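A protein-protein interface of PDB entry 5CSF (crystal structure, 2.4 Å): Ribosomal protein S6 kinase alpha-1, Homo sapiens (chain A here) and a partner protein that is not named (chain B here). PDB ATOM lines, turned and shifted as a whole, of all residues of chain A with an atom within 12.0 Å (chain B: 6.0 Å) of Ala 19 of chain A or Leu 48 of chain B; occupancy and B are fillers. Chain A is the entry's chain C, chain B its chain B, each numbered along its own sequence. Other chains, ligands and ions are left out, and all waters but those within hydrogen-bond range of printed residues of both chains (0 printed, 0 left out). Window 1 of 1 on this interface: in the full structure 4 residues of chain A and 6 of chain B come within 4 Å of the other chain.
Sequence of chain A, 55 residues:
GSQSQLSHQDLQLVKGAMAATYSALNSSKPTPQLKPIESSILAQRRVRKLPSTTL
Of the 11 printed residues of chain B, 4 touch a printed residue of chain A.
Hydrophobic or aromatic side chains of chain A within 4 Å of the printed part of chain B: Met 18 and Ala 19.
Among the printed residues, no Asp or Glu carboxylate lies within 4 Å of a Lys or Arg side-chain nitrogen of the other chain.
O of Phe 47 of chain B is in hydrogen-bond range of N of Ala 19 of chain A (3.2 Å).
The backbone NH (N) of Glu 49 of chain B sits at hydrogen-bond distance from the backbone carbonyl oxygen (O) of Ala 19 of chain A, at 3.1 Å.
Met 18 of chain A touches His 46 of chain B.
CG of Met 18 of chain A touches O of Phe 47 of chain B, at 3.2 Å.
Met 18 of chain A touches Leu 48 of chain B.
O of Ala 19 of chain A touches CA of Leu 48 of chain B (3.95 Å).
Of chain B, only Phe 47 (3.2 Å), Leu 48 (3.95 Å) and Glu 49 (3.1 Å) come within 4 Å of Ala 19 of chain A.
No residue of chain A comes within 4 Å of Ile 40 of chain B.
No residue of chain A comes within 4 Å of Leu 44 of chain B.
Of chain A, only Met 18 and Ala 19 come within 4 Å of Phe 47 of chain B.
Printed residues of chain A within 4 Å of Glu 49 of chain B: Ala 19.
No residue of chain A comes within 4 Å of Val 84 of chain B.
No residue of chain A comes within 4 Å of Ala 87 of chain B.
Printed residues of chain A within 4 Å of His 46 of chain B: Met 18 (3.8 Å).
Printed residues of chain B within 4 Å of Met 18 of chain A: His 46 (3.8 Å), Phe 47 (3.2 Å) and Leu 48 (3.98 Å).
Ala 24 of chain A touches none of the printed residues of chain B.
The nearest residue of chain B that does not touch Ala 19 of chain A is Ala 87 of chain B (5.6 Å).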
ATOM      1  N   ALA A  17     -13.641   1.106  -8.064  1.00  0.00           N
ATOM      2  CA  ALA A  17     -12.894   2.176  -7.406  1.00  0.00           C
ATOM      3  C   ALA A  17     -13.392   3.550  -7.858  1.00  0.00           C
ATOM      4  O   ALA A  17     -13.131   3.950  -8.993  1.00  0.00           O
ATOM      5  CB  ALA A  17     -11.408   2.033  -7.694  1.00  0.00           C
ATOM      6  N   MET A  18     -14.077   4.290  -6.982  1.00  0.00           N
ATOM      7  CA  MET A  18     -14.238   3.935  -5.573  1.00  0.00           C
ATOM      8  C   MET A  18     -15.496   4.560  -4.945  1.00  0.00           C
ATOM      9  O   MET A  18     -16.422   4.967  -5.652  1.00  0.00           O
ATOM     10  CB  MET A  18     -13.001   4.374  -4.786  1.00  0.00           C
ATOM     11  CG  MET A  18     -12.571   3.384  -3.733  1.00  0.00           C
ATOM     12  SD  MET A  18     -10.861   3.618  -3.219  1.00  0.00           S
ATOM     13  CE  MET A  18      -9.948   2.946  -4.614  1.00  0.00           C
ATOM     14  N   ALA A  19     -15.514   4.640  -3.614  1.00  0.00           N
ATOM     15  CA  ALA A  19     -16.606   5.270  -2.872  1.00  0.00           C
ATOM     16  C   ALA A  19     -16.097   6.037  -1.642  1.00  0.00           C
ATOM     17  O   ALA A  19     -14.893   6.209  -1.446  1.00  0.00           O
ATOM     18  CB  ALA A  19     -17.629   4.228  -2.452  1.00  0.00           C
ATOM     19  N   ALA A  20     -17.034   6.501  -0.822  1.00  0.00           N
ATOM     20  CA  ALA A  20     -16.722   7.187   0.433  1.00  0.00           C
ATOM     21  C   ALA A  20     -17.999   7.279   1.278  1.00  0.00           C
ATOM     22  O   ALA A  20     -18.999   6.608   0.979  1.00  0.00           O
ATOM     23  CB  ALA A  20     -16.146   8.569   0.171  1.00  0.00           C
ATOM     24  N   THR A  21     -17.973   8.115   2.317  1.00  0.00           N
ATOM     25  CA  THR A  21     -19.113   8.276   3.232  1.00  0.00           C
ATOM     26  C   THR A  21     -20.447   8.704   2.556  1.00  0.00           C
ATOM     27  O   THR A  21     -20.712   9.900   2.386  1.00  0.00           O
ATOM     28  CB  THR A  21     -18.757   9.299   4.358  1.00  0.00           C
ATOM     29  OG1 THR A  21     -19.947   9.939   4.843  1.00  0.00           O
ATOM     30  CG2 THR A  21     -17.772  10.359   3.848  1.00  0.00           C
ATOM     31  N   TYR A  22     -21.279   7.720   2.190  1.00  0.00           N
ATOM     32  CA  TYR A  22     -22.608   7.967   1.608  1.00  0.00           C
ATOM     33  C   TYR A  22     -23.719   7.531   2.566  1.00  0.00           C
ATOM     34  O   TYR A  22     -24.581   8.338   2.947  1.00  0.00           O
ATOM     35  CB  TYR A  22     -22.751   7.242   0.269  1.00  0.00           C
ATOM     36  N   SER A  23     -23.712   6.250   2.930  1.00  0.00           N
ATOM     37  CA  SER A  23     -24.521   5.753   4.049  1.00  0.00           C
ATOM     38  C   SER A  23     -26.027   5.924   3.859  1.00  0.00           C
ATOM     39  O   SER A  23     -26.605   6.913   4.333  1.00  0.00           O
ATOM     40  CB  SER A  23     -24.096   6.449   5.343  1.00  0.00           C
ATOM     41  N   ALA A  24     -26.653   4.955   3.182  1.00  0.00           N
ATOM     42  CA  ALA A  24     -28.108   4.895   3.050  1.00  0.00           C
ATOM     43  C   ALA A  24     -28.708   3.916   4.066  1.00  0.00           C
ATOM     44  O   ALA A  24     -29.415   2.967   3.693  1.00  0.00           O
ATOM     45  CB  ALA A  24     -28.493   4.497   1.630  1.00  0.00           C
ATOM     46  N   ILE B  40     -11.410   0.215   8.444  1.00  0.00           N
ATOM     47  CA  ILE B  40     -11.729   0.714   7.104  1.00  0.00           C
ATOM     48  C   ILE B  40     -10.467   0.921   6.290  1.00  0.00           C
ATOM     49  O   ILE B  40     -10.404   0.549   5.109  1.00  0.00           O
ATOM     50  CB  ILE B  40     -12.554   2.008   7.164  1.00  0.00           C
ATOM     51  CG1 ILE B  40     -13.967   1.668   7.665  1.00  0.00           C
ATOM     52  CG2 ILE B  40     -12.636   2.657   5.791  1.00  0.00           C
ATOM     53  CD1 ILE B  40     -14.854   2.873   7.936  1.00  0.00           C
ATOM     54  N   LEU B  44     -10.516  -2.228   3.982  1.00  0.00           N
ATOM     55  CA  LEU B  44     -11.439  -1.796   2.935  1.00  0.00           C
ATOM     56  C   LEU B  44     -10.747  -0.783   2.029  1.00  0.00           C
ATOM     57  O   LEU B  44     -11.402   0.025   1.375  1.00  0.00           O
ATOM     58  CB  LEU B  44     -12.711  -1.182   3.527  1.00  0.00           C
ATOM     59  CG  LEU B  44     -13.685  -2.181   4.145  1.00  0.00           C
ATOM     60  CD1 LEU B  44     -14.818  -1.424   4.808  1.00  0.00           C
ATOM     61  CD2 LEU B  44     -14.206  -3.180   3.106  1.00  0.00           C
ATOM     62  N   SER B  45      -9.431  -0.874   1.918  1.00  0.00           N
ATOM     63  CA  SER B  45      -8.661   0.159   1.221  1.00  0.00           C
ATOM     64  C   SER B  45      -8.964   0.238  -0.282  1.00  0.00           C
ATOM     65  O   SER B  45      -8.606   1.229  -0.931  1.00  0.00           O
ATOM     66  CB  SER B  45      -7.169  -0.058   1.475  1.00  0.00           C
ATOM     67  OG  SER B  45      -6.689  -1.266   0.911  1.00  0.00           O
ATOM     68  N   HIS B  46      -9.530  -0.835  -0.836  1.00  0.00           N
ATOM     69  CA  HIS B  46      -9.928  -0.871  -2.255  1.00  0.00           C
ATOM     70  C   HIS B  46     -11.383  -0.475  -2.533  1.00  0.00           C
ATOM     71  O   HIS B  46     -11.762  -0.305  -3.691  1.00  0.00           O
ATOM     72  CB  HIS B  46      -9.702  -2.255  -2.863  1.00  0.00           C
ATOM     73  CG  HIS B  46      -8.320  -2.773  -2.654  1.00  0.00           C
ATOM     74  ND1 HIS B  46      -7.985  -3.590  -1.597  1.00  0.00           N
ATOM     75  CD2 HIS B  46      -7.160  -2.489  -3.292  1.00  0.00           C
ATOM     76  CE1 HIS B  46      -6.688  -3.845  -1.637  1.00  0.00           C
ATOM     77  NE2 HIS B  46      -6.162  -3.177  -2.648  1.00  0.00           N
ATOM     78  N   PHE B  47     -12.199  -0.343  -1.489  1.00  0.00           N
ATOM     79  CA  PHE B  47     -13.605  -0.002  -1.690  1.00  0.00           C
ATOM     80  C   PHE B  47     -13.898   1.413  -1.136  1.00  0.00           C
ATOM     81  O   PHE B  47     -14.691   2.156  -1.717  1.00  0.00           O
ATOM     82  CB  PHE B  47     -14.529  -1.043  -1.043  1.00  0.00           C
ATOM     83  CG  PHE B  47     -14.440  -2.420  -1.675  1.00  0.00           C
ATOM     84  CD1 PHE B  47     -13.818  -2.606  -2.909  1.00  0.00           C
ATOM     85  CD2 PHE B  47     -15.050  -3.517  -1.078  1.00  0.00           C
ATOM     86  CE1 PHE B  47     -13.737  -3.875  -3.504  1.00  0.00           C
ATOM     87  CE2 PHE B  47     -15.000  -4.790  -1.677  1.00  0.00           C
ATOM     88  CZ  PHE B  47     -14.331  -4.966  -2.886  1.00  0.00           C
ATOM     89  N   LEU B  48     -13.317   1.762   0.014  1.00  0.00           N
ATOM     90  CA  LEU B  48     -13.512   3.103   0.567  1.00  0.00           C
ATOM     91  C   LEU B  48     -12.259   3.978   0.520  1.00  0.00           C
ATOM     92  O   LEU B  48     -11.127   3.529   0.750  1.00  0.00           O
ATOM     93  CB  LEU B  48     -14.024   3.003   2.004  1.00  0.00           C
ATOM     94  CG  LEU B  48     -15.308   2.185   2.158  1.00  0.00           C
ATOM     95  CD1 LEU B  48     -15.759   2.151   3.591  1.00  0.00           C
ATOM     96  CD2 LEU B  48     -16.391   2.787   1.286  1.00  0.00           C
ATOM     97  N   GLU B  49     -12.477   5.261   0.276  1.00  0.00           N
ATOM     98  CA  GLU B  49     -11.387   6.200   0.326  1.00  0.00           C
ATOM     99  C   GLU B  49     -10.871   6.201   1.759  1.00  0.00           C
ATOM    100  O   GLU B  49     -11.654   6.038   2.695  1.00  0.00           O
ATOM    101  CB  GLU B  49     -11.879   7.567  -0.146  1.00  0.00           C
ATOM    102  CG  GLU B  49     -10.819   8.448  -0.780  1.00  0.00           C
ATOM    103  CD  GLU B  49     -11.397   9.328  -1.879  1.00  0.00           C
ATOM    104  OE1 GLU B  49     -10.785  10.373  -2.187  1.00  0.00           O
ATOM    105  OE2 GLU B  49     -12.452   8.951  -2.455  1.00  0.00           O
ATOM    106  N   GLU B  50      -9.560   6.346   1.925  1.00  0.00           N
ATOM    107  CA  GLU B  50      -8.957   6.322   3.250  1.00  0.00           C
ATOM    108  C   GLU B  50      -9.587   7.366   4.159  1.00  0.00           C
ATOM    109  O   GLU B  50      -9.998   8.423   3.694  1.00  0.00           O
ATOM    110  CB  GLU B  50      -7.452   6.519   3.146  1.00  0.00           C
ATOM    111  CG  GLU B  50      -6.717   6.406   4.447  1.00  0.00           C
ATOM    112  CD  GLU B  50      -5.217   6.466   4.249  1.00  0.00           C
ATOM    113  OE1 GLU B  50      -4.782   6.854   3.140  1.00  0.00           O
ATOM    114  OE2 GLU B  50      -4.477   6.149   5.204  1.00  0.00           O
ATOM    115  N   PHE B  80     -23.393  -2.247   8.181  1.00  0.00           N
ATOM    116  CA  PHE B  80     -22.331  -1.522   7.481  1.00  0.00           C
ATOM    117  C   PHE B  80     -21.822  -2.331   6.295  1.00  0.00           C
ATOM    118  O   PHE B  80     -21.636  -1.786   5.212  1.00  0.00           O
ATOM    119  CB  PHE B  80     -21.188  -1.164   8.446  1.00  0.00           C
ATOM    120  CG  PHE B  80     -20.038  -0.445   7.796  1.00  0.00           C
ATOM    121  CD1 PHE B  80     -20.218   0.807   7.218  1.00  0.00           C
ATOM    122  CD2 PHE B  80     -18.757  -0.989   7.804  1.00  0.00           C
ATOM    123  CE1 PHE B  80     -19.127   1.490   6.618  1.00  0.00           C
ATOM    124  CE2 PHE B  80     -17.674  -0.314   7.205  1.00  0.00           C
ATOM    125  CZ  PHE B  80     -17.869   0.931   6.620  1.00  0.00           C
ATOM    126  N   VAL B  84     -21.958  -1.375   2.258  1.00  0.00           N
ATOM    127  CA  VAL B  84     -20.773  -1.314   1.398  1.00  0.00           C
ATOM    128  C   VAL B  84     -20.919  -2.289   0.230  1.00  0.00           C
ATOM    129  O   VAL B  84     -20.675  -1.903  -0.906  1.00  0.00           O
ATOM    130  CB  VAL B  84     -19.474  -1.623   2.180  1.00  0.00           C
ATOM    131  CG1 VAL B  84     -18.221  -1.496   1.278  1.00  0.00           C
ATOM    132  CG2 VAL B  84     -19.348  -0.695   3.384  1.00  0.00           C
ATOM    133  N   ALA B  87     -23.428  -1.143  -2.548  1.00  0.00           N
ATOM    134  CA  ALA B  87     -22.918  -0.075  -3.414  1.00  0.00           C
ATOM    135  C   ALA B  87     -21.953  -0.598  -4.489  1.00  0.00           C
ATOM    136  O   ALA B  87     -21.992  -0.183  -5.649  1.00  0.00           O
ATOM    137  CB  ALA B  87     -22.249   1.004  -2.584  1.00  0.00           C
